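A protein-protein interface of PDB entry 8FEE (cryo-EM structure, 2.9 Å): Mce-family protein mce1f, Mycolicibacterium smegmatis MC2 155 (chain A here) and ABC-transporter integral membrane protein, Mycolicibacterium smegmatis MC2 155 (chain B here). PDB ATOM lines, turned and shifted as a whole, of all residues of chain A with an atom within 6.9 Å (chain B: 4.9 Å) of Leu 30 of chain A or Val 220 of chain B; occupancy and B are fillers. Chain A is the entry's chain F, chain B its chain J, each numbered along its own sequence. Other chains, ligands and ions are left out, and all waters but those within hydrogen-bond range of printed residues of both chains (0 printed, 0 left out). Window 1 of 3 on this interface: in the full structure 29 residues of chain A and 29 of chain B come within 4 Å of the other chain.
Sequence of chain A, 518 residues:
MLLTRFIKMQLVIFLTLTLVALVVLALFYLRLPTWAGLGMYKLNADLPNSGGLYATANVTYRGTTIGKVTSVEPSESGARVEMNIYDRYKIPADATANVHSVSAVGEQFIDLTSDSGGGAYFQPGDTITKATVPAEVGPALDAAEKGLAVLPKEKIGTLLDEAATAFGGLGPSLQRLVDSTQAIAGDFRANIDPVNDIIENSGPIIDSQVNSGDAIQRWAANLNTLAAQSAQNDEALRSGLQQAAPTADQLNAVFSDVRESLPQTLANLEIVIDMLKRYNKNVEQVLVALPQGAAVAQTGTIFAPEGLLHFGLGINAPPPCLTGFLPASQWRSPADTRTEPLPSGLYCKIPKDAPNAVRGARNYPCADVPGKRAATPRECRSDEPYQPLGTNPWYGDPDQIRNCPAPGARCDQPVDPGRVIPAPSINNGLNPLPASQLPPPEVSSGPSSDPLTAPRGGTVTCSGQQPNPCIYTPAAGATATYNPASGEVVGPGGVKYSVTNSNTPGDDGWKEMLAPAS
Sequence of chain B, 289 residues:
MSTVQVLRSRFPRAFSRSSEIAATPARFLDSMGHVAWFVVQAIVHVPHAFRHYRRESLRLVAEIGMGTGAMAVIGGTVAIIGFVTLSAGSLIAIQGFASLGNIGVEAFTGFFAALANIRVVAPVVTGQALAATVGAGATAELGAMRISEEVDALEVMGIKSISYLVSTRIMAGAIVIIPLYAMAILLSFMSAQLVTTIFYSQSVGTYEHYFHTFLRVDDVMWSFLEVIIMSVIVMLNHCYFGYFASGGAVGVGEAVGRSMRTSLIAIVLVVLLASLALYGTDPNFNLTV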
ATOM      1  N   VAL A  24      18.185 -33.734  -8.671  1.00  0.00           N
ATOM      2  CA  VAL A  24      17.262 -33.065  -9.584  1.00  0.00           C
ATOM      3  C   VAL A  24      16.114 -32.416  -8.817  1.00  0.00           C
ATOM      4  O   VAL A  24      15.712 -31.286  -9.118  1.00  0.00           O
ATOM      5  CB  VAL A  24      16.756 -34.057 -10.648  1.00  0.00           C
ATOM      6  CG1 VAL A  24      15.583 -33.473 -11.415  1.00  0.00           C
ATOM      7  CG2 VAL A  24      17.880 -34.415 -11.606  1.00  0.00           C
ATOM      8  N   LEU A  25      15.574 -33.108  -7.810  1.00  0.00           N
ATOM      9  CA  LEU A  25      14.483 -32.540  -7.025  1.00  0.00           C
ATOM     10  C   LEU A  25      14.944 -31.347  -6.195  1.00  0.00           C
ATOM     11  O   LEU A  25      14.195 -30.377  -6.029  1.00  0.00           O
ATOM     12  CB  LEU A  25      13.873 -33.616  -6.127  1.00  0.00           C
ATOM     13  CG  LEU A  25      12.692 -33.188  -5.257  1.00  0.00           C
ATOM     14  CD1 LEU A  25      11.537 -32.732  -6.125  1.00  0.00           C
ATOM     15  CD2 LEU A  25      12.262 -34.319  -4.342  1.00  0.00           C
ATOM     16  N   ALA A  26      16.171 -31.389  -5.673  1.00  0.00           N
ATOM     17  CA  ALA A  26      16.654 -30.302  -4.832  1.00  0.00           C
ATOM     18  C   ALA A  26      17.101 -29.086  -5.633  1.00  0.00           C
ATOM     19  O   ALA A  26      16.990 -27.958  -5.143  1.00  0.00           O
ATOM     20  CB  ALA A  26      17.804 -30.795  -3.954  1.00  0.00           C
ATOM     21  N   LEU A  27      17.608 -29.280  -6.849  1.00  0.00           N
ATOM     22  CA  LEU A  27      18.111 -28.153  -7.629  1.00  0.00           C
ATOM     23  C   LEU A  27      17.039 -27.543  -8.529  1.00  0.00           C
ATOM     24  O   LEU A  27      16.748 -26.347  -8.434  1.00  0.00           O
ATOM     25  CB  LEU A  27      19.319 -28.591  -8.464  1.00  0.00           C
ATOM     26  CG  LEU A  27      20.608 -28.889  -7.700  1.00  0.00           C
ATOM     27  CD1 LEU A  27      21.722 -29.259  -8.663  1.00  0.00           C
ATOM     28  CD2 LEU A  27      21.014 -27.702  -6.843  1.00  0.00           C
ATOM     29  N   PHE A  28      16.445 -28.351  -9.404  1.00  0.00           N
ATOM     30  CA  PHE A  28      15.580 -27.834 -10.456  1.00  0.00           C
ATOM     31  C   PHE A  28      14.114 -27.730 -10.055  1.00  0.00           C
ATOM     32  O   PHE A  28      13.346 -27.069 -10.763  1.00  0.00           O
ATOM     33  CB  PHE A  28      15.700 -28.709 -11.707  1.00  0.00           C
ATOM     34  CG  PHE A  28      17.099 -28.808 -12.244  1.00  0.00           C
ATOM     35  CD1 PHE A  28      17.594 -27.844 -13.105  1.00  0.00           C
ATOM     36  CD2 PHE A  28      17.918 -29.866 -11.888  1.00  0.00           C
ATOM     37  CE1 PHE A  28      18.882 -27.932 -13.601  1.00  0.00           C
ATOM     38  CE2 PHE A  28      19.206 -29.960 -12.380  1.00  0.00           C
ATOM     39  CZ  PHE A  28      19.688 -28.993 -13.237  1.00  0.00           C
ATOM     40  N   TYR A  29      13.702 -28.349  -8.957  1.00  0.00           N
ATOM     41  CA  TYR A  29      12.291 -28.357  -8.585  1.00  0.00           C
ATOM     42  C   TYR A  29      12.003 -27.681  -7.256  1.00  0.00           C
ATOM     43  O   TYR A  29      11.012 -26.955  -7.147  1.00  0.00           O
ATOM     44  CB  TYR A  29      11.765 -29.797  -8.550  1.00  0.00           C
ATOM     45  CG  TYR A  29      11.402 -30.337  -9.914  1.00  0.00           C
ATOM     46  CD1 TYR A  29      12.386 -30.709 -10.819  1.00  0.00           C
ATOM     47  CD2 TYR A  29      10.075 -30.473 -10.297  1.00  0.00           C
ATOM     48  CE1 TYR A  29      12.059 -31.200 -12.068  1.00  0.00           C
ATOM     49  CE2 TYR A  29       9.739 -30.963 -11.543  1.00  0.00           C
ATOM     50  CZ  TYR A  29      10.735 -31.326 -12.423  1.00  0.00           C
ATOM     51  OH  TYR A  29      10.404 -31.815 -13.665  1.00  0.00           O
ATOM     52  N   LEU A  30      12.833 -27.899  -6.238  1.00  0.00           N
ATOM     53  CA  LEU A  30      12.633 -27.255  -4.947  1.00  0.00           C
ATOM     54  C   LEU A  30      13.480 -26.006  -4.755  1.00  0.00           C
ATOM     55  O   LEU A  30      13.110 -25.152  -3.941  1.00  0.00           O
ATOM     56  CB  LEU A  30      12.929 -28.237  -3.809  1.00  0.00           C
ATOM     57  CG  LEU A  30      12.017 -29.460  -3.719  1.00  0.00           C
ATOM     58  CD1 LEU A  30      12.348 -30.279  -2.486  1.00  0.00           C
ATOM     59  CD2 LEU A  30      10.560 -29.036  -3.713  1.00  0.00           C
ATOM     60  N   ARG A  31      14.595 -25.886  -5.478  1.00  0.00           N
ATOM     61  CA  ARG A  31      15.524 -24.763  -5.354  1.00  0.00           C
ATOM     62  C   ARG A  31      16.026 -24.618  -3.916  1.00  0.00           C
ATOM     63  O   ARG A  31      15.839 -23.590  -3.261  1.00  0.00           O
ATOM     64  CB  ARG A  31      14.894 -23.459  -5.858  1.00  0.00           C
ATOM     65  CG  ARG A  31      14.610 -23.440  -7.349  1.00  0.00           C
ATOM     66  CD  ARG A  31      14.045 -22.099  -7.779  1.00  0.00           C
ATOM     67  NE  ARG A  31      13.851 -22.027  -9.222  1.00  0.00           N
ATOM     68  CZ  ARG A  31      13.471 -20.935  -9.873  1.00  0.00           C
ATOM     69  NH1 ARG A  31      13.238 -19.799  -9.239  1.00  0.00           N
ATOM     70  NH2 ARG A  31      13.322 -20.987 -11.194  1.00  0.00           N
ATOM     71  N   LEU A  32      16.655 -25.686  -3.428  1.00  0.00           N
ATOM     72  CA  LEU A  32      17.259 -25.642  -2.099  1.00  0.00           C
ATOM     73  C   LEU A  32      18.325 -24.561  -1.935  1.00  0.00           C
ATOM     74  O   LEU A  32      18.368 -23.952  -0.852  1.00  0.00           O
ATOM     75  CB  LEU A  32      17.830 -27.019  -1.734  1.00  0.00           C
ATOM     76  CG  LEU A  32      16.820 -28.070  -1.276  1.00  0.00           C
ATOM     77  CD1 LEU A  32      17.531 -29.253  -0.648  1.00  0.00           C
ATOM     78  CD2 LEU A  32      15.842 -27.458  -0.297  1.00  0.00           C
ATOM     79  N   PRO A  33      19.222 -24.296  -2.898  1.00  0.00           N
ATOM     80  CA  PRO A  33      20.152 -23.168  -2.708  1.00  0.00           C
ATOM     81  C   PRO A  33      19.453 -21.834  -2.511  1.00  0.00           C
ATOM     82  O   PRO A  33      19.957 -20.983  -1.766  1.00  0.00           O
ATOM     83  CB  PRO A  33      20.992 -23.184  -3.992  1.00  0.00           C
ATOM     84  CG  PRO A  33      20.947 -24.584  -4.442  1.00  0.00           C
ATOM     85  CD  PRO A  33      19.576 -25.074  -4.103  1.00  0.00           C
ATOM     86  N   THR A  34      18.306 -21.625  -3.160  1.00  0.00           N
ATOM     87  CA  THR A  34      17.555 -20.390  -2.968  1.00  0.00           C
ATOM     88  C   THR A  34      16.828 -20.377  -1.627  1.00  0.00           C
ATOM     89  O   THR A  34      16.804 -19.349  -0.942  1.00  0.00           O
ATOM     90  CB  THR A  34      16.564 -20.203  -4.121  1.00  0.00           C
ATOM     91  OG1 THR A  34      17.285 -19.995  -5.342  1.00  0.00           O
ATOM     92  CG2 THR A  34      15.651 -19.013  -3.871  1.00  0.00           C
ATOM     93  N   TRP A  35      16.235 -21.508  -1.234  1.00  0.00           N
ATOM     94  CA  TRP A  35      15.532 -21.566   0.044  1.00  0.00           C
ATOM     95  C   TRP A  35      16.489 -21.367   1.213  1.00  0.00           C
ATOM     96  O   TRP A  35      16.169 -20.658   2.174  1.00  0.00           O
ATOM     97  CB  TRP A  35      14.790 -22.894   0.174  1.00  0.00           C
ATOM     98  CG  TRP A  35      14.120 -23.080   1.498  1.00  0.00           C
ATOM     99  CD1 TRP A  35      12.929 -22.547   1.894  1.00  0.00           C
ATOM    100  CD2 TRP A  35      14.597 -23.859   2.601  1.00  0.00           C
ATOM    101  NE1 TRP A  35      12.636 -22.943   3.176  1.00  0.00           N
ATOM    102  CE2 TRP A  35      13.645 -23.750   3.632  1.00  0.00           C
ATOM    103  CE3 TRP A  35      15.739 -24.638   2.816  1.00  0.00           C
ATOM    104  CZ2 TRP A  35      13.799 -24.390   4.860  1.00  0.00           C
ATOM    105  CZ3 TRP A  35      15.889 -25.272   4.036  1.00  0.00           C
ATOM    106  CH2 TRP A  35      14.924 -25.144   5.042  1.00  0.00           C
ATOM    107  N   ILE B 118       1.701 -31.863  -2.897  1.00  0.00           N
ATOM    108  CA  ILE B 118       2.382 -31.989  -1.611  1.00  0.00           C
ATOM    109  C   ILE B 118       1.393 -32.284  -0.491  1.00  0.00           C
ATOM    110  O   ILE B 118       1.661 -33.104   0.394  1.00  0.00           O
ATOM    111  CB  ILE B 118       3.198 -30.716  -1.323  1.00  0.00           C
ATOM    112  CG1 ILE B 118       4.333 -30.579  -2.333  1.00  0.00           C
ATOM    113  CG2 ILE B 118       3.758 -30.741   0.086  1.00  0.00           C
ATOM    114  CD1 ILE B 118       5.269 -31.757  -2.334  1.00  0.00           C
ATOM    115  N   PHE B 189       5.399 -33.972 -10.038  1.00  0.00           N
ATOM    116  CA  PHE B 189       5.620 -32.606 -10.506  1.00  0.00           C
ATOM    117  C   PHE B 189       5.855 -32.570 -12.009  1.00  0.00           C
ATOM    118  O   PHE B 189       5.292 -31.721 -12.715  1.00  0.00           O
ATOM    119  CB  PHE B 189       6.804 -31.975  -9.773  1.00  0.00           C
ATOM    120  CG  PHE B 189       6.523 -31.624  -8.341  1.00  0.00           C
ATOM    121  CD1 PHE B 189       5.229 -31.613  -7.853  1.00  0.00           C
ATOM    122  CD2 PHE B 189       7.557 -31.289  -7.485  1.00  0.00           C
ATOM    123  CE1 PHE B 189       4.974 -31.285  -6.538  1.00  0.00           C
ATOM    124  CE2 PHE B 189       7.307 -30.960  -6.171  1.00  0.00           C
ATOM    125  CZ  PHE B 189       6.014 -30.959  -5.698  1.00  0.00           C
ATOM    126  N   LEU B 215       5.135 -22.541  -3.754  1.00  0.00           N
ATOM    127  CA  LEU B 215       5.542 -23.805  -3.157  1.00  0.00           C
ATOM    128  C   LEU B 215       6.544 -23.537  -2.045  1.00  0.00           C
ATOM    129  O   LEU B 215       7.541 -22.839  -2.258  1.00  0.00           O
ATOM    130  CB  LEU B 215       6.155 -24.743  -4.197  1.00  0.00           C
ATOM    131  CG  LEU B 215       6.616 -26.111  -3.689  1.00  0.00           C
ATOM    132  CD1 LEU B 215       5.427 -27.035  -3.482  1.00  0.00           C
ATOM    133  CD2 LEU B 215       7.623 -26.729  -4.641  1.00  0.00           C
ATOM    134  N   ARG B 216       6.282 -24.092  -0.866  1.00  0.00           N
ATOM    135  CA  ARG B 216       7.164 -23.962   0.284  1.00  0.00           C
ATOM    136  C   ARG B 216       7.895 -25.277   0.511  1.00  0.00           C
ATOM    137  O   ARG B 216       7.263 -26.334   0.604  1.00  0.00           O
ATOM    138  CB  ARG B 216       6.384 -23.559   1.537  1.00  0.00           C
ATOM    139  CG  ARG B 216       6.249 -22.055   1.728  1.00  0.00           C
ATOM    140  CD  ARG B 216       5.153 -21.466   0.858  1.00  0.00           C
ATOM    141  NE  ARG B 216       5.137 -20.009   0.922  1.00  0.00           N
ATOM    142  CZ  ARG B 216       4.517 -19.305   1.860  1.00  0.00           C
ATOM    143  NH1 ARG B 216       3.845 -19.894   2.835  1.00  0.00           N
ATOM    144  NH2 ARG B 216       4.574 -17.978   1.819  1.00  0.00           N
ATOM    145  N   VAL B 217       9.227 -25.207   0.597  1.00  0.00           N
ATOM    146  CA  VAL B 217      10.037 -26.389   0.871  1.00  0.00           C
ATOM    147  C   VAL B 217       9.729 -26.967   2.247  1.00  0.00           C
ATOM    148  O   VAL B 217       9.929 -28.167   2.477  1.00  0.00           O
ATOM    149  CB  VAL B 217      11.532 -26.027   0.724  1.00  0.00           C
ATOM    150  CG1 VAL B 217      12.412 -27.254   0.870  1.00  0.00           C
ATOM    151  CG2 VAL B 217      11.778 -25.351  -0.613  1.00  0.00           C
ATOM    152  N   ASP B 218       9.222 -26.142   3.166  1.00  0.00           N
ATOM    153  CA  ASP B 218       8.802 -26.641   4.469  1.00  0.00           C
ATOM    154  C   ASP B 218       7.694 -27.676   4.325  1.00  0.00           C
ATOM    155  O   ASP B 218       7.694 -28.703   5.018  1.00  0.00           O
ATOM    156  CB  ASP B 218       8.343 -25.475   5.344  1.00  0.00           C
ATOM    157  CG  ASP B 218       7.832 -25.924   6.694  1.00  0.00           C
ATOM    158  OD1 ASP B 218       8.657 -26.341   7.534  1.00  0.00           O
ATOM    159  OD2 ASP B 218       6.605 -25.861   6.917  1.00  0.00           O
ATOM    160  N   ASP B 219       6.749 -27.427   3.413  1.00  0.00           N
ATOM    161  CA  ASP B 219       5.693 -28.397   3.146  1.00  0.00           C
ATOM    162  C   ASP B 219       6.270 -29.711   2.641  1.00  0.00           C
ATOM    163  O   ASP B 219       5.833 -30.789   3.057  1.00  0.00           O
ATOM    164  CB  ASP B 219       4.703 -27.826   2.131  1.00  0.00           C
ATOM    165  CG  ASP B 219       4.007 -26.581   2.632  1.00  0.00           C
ATOM    166  OD1 ASP B 219       3.751 -26.493   3.850  1.00  0.00           O
ATOM    167  OD2 ASP B 219       3.713 -25.691   1.808  1.00  0.00           O
ATOM    168  N   VAL B 220       7.262 -29.639   1.750  1.00  0.00           N
ATOM    169  CA  VAL B 220       7.868 -30.846   1.199  1.00  0.00           C
ATOM    170  C   VAL B 220       8.586 -31.635   2.289  1.00  0.00           C
ATOM    171  O   VAL B 220       8.484 -32.866   2.350  1.00  0.00           O
ATOM    172  CB  VAL B 220       8.816 -30.479   0.042  1.00  0.00           C
ATOM    173  CG1 VAL B 220       9.487 -31.721  -0.518  1.00  0.00           C
ATOM    174  CG2 VAL B 220       8.061 -29.738  -1.045  1.00  0.00           C
ATOM    175  N   MET B 221       9.329 -30.946   3.161  1.00  0.00           N
ATOM    176  CA  MET B 221      10.040 -31.642   4.231  1.00  0.00           C
ATOM    177  C   MET B 221       9.074 -32.297   5.213  1.00  0.00           C
ATOM    178  O   MET B 221       9.273 -33.454   5.618  1.00  0.00           O
ATOM    179  CB  MET B 221      10.971 -30.674   4.959  1.00  0.00           C
ATOM    180  CG  MET B 221      12.095 -30.132   4.094  1.00  0.00           C
ATOM    181  SD  MET B 221      13.202 -29.036   5.000  1.00  0.00           S
ATOM    182  CE  MET B 221      13.866 -30.165   6.221  1.00  0.00           C
ATOM    183  N   TRP B 222       8.019 -31.579   5.610  1.00  0.00           N
ATOM    184  CA  TRP B 222       7.048 -32.188   6.510  1.00  0.00           C
ATOM    185  C   TRP B 222       6.312 -33.342   5.842  1.00  0.00           C
ATOM    186  O   TRP B 222       5.994 -34.334   6.506  1.00  0.00           O
ATOM    187  CB  TRP B 222       6.061 -31.142   7.023  1.00  0.00           C
ATOM    188  CG  TRP B 222       6.659 -30.184   8.015  1.00  0.00           C
ATOM    189  CD1 TRP B 222       6.817 -28.840   7.861  1.00  0.00           C
ATOM    190  CD2 TRP B 222       7.183 -30.502   9.311  1.00  0.00           C
ATOM    191  NE1 TRP B 222       7.404 -28.299   8.979  1.00  0.00           N
ATOM    192  CE2 TRP B 222       7.639 -29.300   9.884  1.00  0.00           C
ATOM    193  CE3 TRP B 222       7.309 -31.686  10.043  1.00  0.00           C
ATOM    194  CZ2 TRP B 222       8.211 -29.246  11.152  1.00  0.00           C
ATOM    195  CZ3 TRP B 222       7.878 -31.631  11.302  1.00  0.00           C
ATOM    196  CH2 TRP B 222       8.321 -30.420  11.843  1.00  0.00           C
ATOM    197  N   SER B 223       6.075 -33.254   4.530  1.00  0.00           N
ATOM    198  CA  SER B 223       5.486 -34.372   3.800  1.00  0.00           C
ATOM    199  C   SER B 223       6.415 -35.577   3.797  1.00  0.00           C
ATOM    200  O   SER B 223       5.962 -36.721   3.912  1.00  0.00           O
ATOM    201  CB  SER B 223       5.153 -33.946   2.372  1.00  0.00           C
ATOM    202  OG  SER B 223       4.776 -35.058   1.582  1.00  0.00           O
ATOM    203  N   PHE B 224       7.720 -35.339   3.649  1.00  0.00           N
ATOM    204  CA  PHE B 224       8.691 -36.426   3.725  1.00  0.00           C
ATOM    205  C   PHE B 224       8.644 -37.108   5.087  1.00  0.00           C
ATOM    206  O   PHE B 224       8.701 -38.341   5.175  1.00  0.00           O
ATOM    207  CB  PHE B 224      10.096 -35.899   3.443  1.00  0.00           C
ATOM    208  CG  PHE B 224      10.568 -36.147   2.043  1.00  0.00           C
ATOM    209  CD1 PHE B 224      10.260 -35.260   1.025  1.00  0.00           C
ATOM    210  CD2 PHE B 224      11.330 -37.262   1.744  1.00  0.00           C
ATOM    211  CE1 PHE B 224      10.698 -35.486  -0.264  1.00  0.00           C
ATOM    212  CE2 PHE B 224      11.773 -37.492   0.456  1.00  0.00           C
ATOM    213  CZ  PHE B 224      11.456 -36.602  -0.548  1.00  0.00           C
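The backbone NH (N) of Leu 32 of chain A sits at hydrogen-bond distance from the backbone carbonyl oxygen (O) of Ala 26 of chain A (2.9 Å).
N of Leu 30 of chain A lies within hydrogen-bond range of O of Leu 25 of chain A (2.8 Å).
Phe 189 of chain B touches Tyr 29 of chain A.
Leu 215 of chain B touches Leu 30 of chain A.
Leu 30 of chain A touches Val 217 of chain B (O to CG2, 3.6 Å).
Leu 30 of chain A touches Val 220 of chain B.
Val 217 of chain B touches Leu 32 of chain A (CG1 to CD2, 3.6 Å).
Val 217 of chain B touches Trp 35 of chain A (CG2 to CG, 3.9 Å).
Hydrophobic or aromatic side chains of chain A within 4 Å of the printed part of chain B: Tyr 29, Leu 30, Leu 32 and Trp 35.
Hydrophobic or aromatic side chains of chain B within 4 Å of the printed part of chain A: Phe 189, Leu 215, Val 217 and Val 220.
Among the printed residues, no Asp or Glu carboxylate lies within 4 Å of a Lys or Arg side-chain nitrogen of the other chain.
Of chain B, only Leu 215, Val 217 and Val 220 come within 4 Å of Leu 30 of chain A.
Of the printed residues of chain B, Leu 32 of chain A touches Val 217.
Of the printed residues of chain A, Phe 189 of chain B touches Tyr 29 (3.6 Å).
Of the printed residues of chain A, Leu 215 of chain B touches Leu 30 (3.8 Å).
Printed residues of chain A within 4 Å of Val 217 of chain B: Leu 30, Leu 32 and Trp 35.
Val 220 of chain B touches just one residue of chain A: Leu 30.
The nearest residue of chain A that does not touch Val 220 of chain B is Leu 25 of chain A (5.4 Å).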
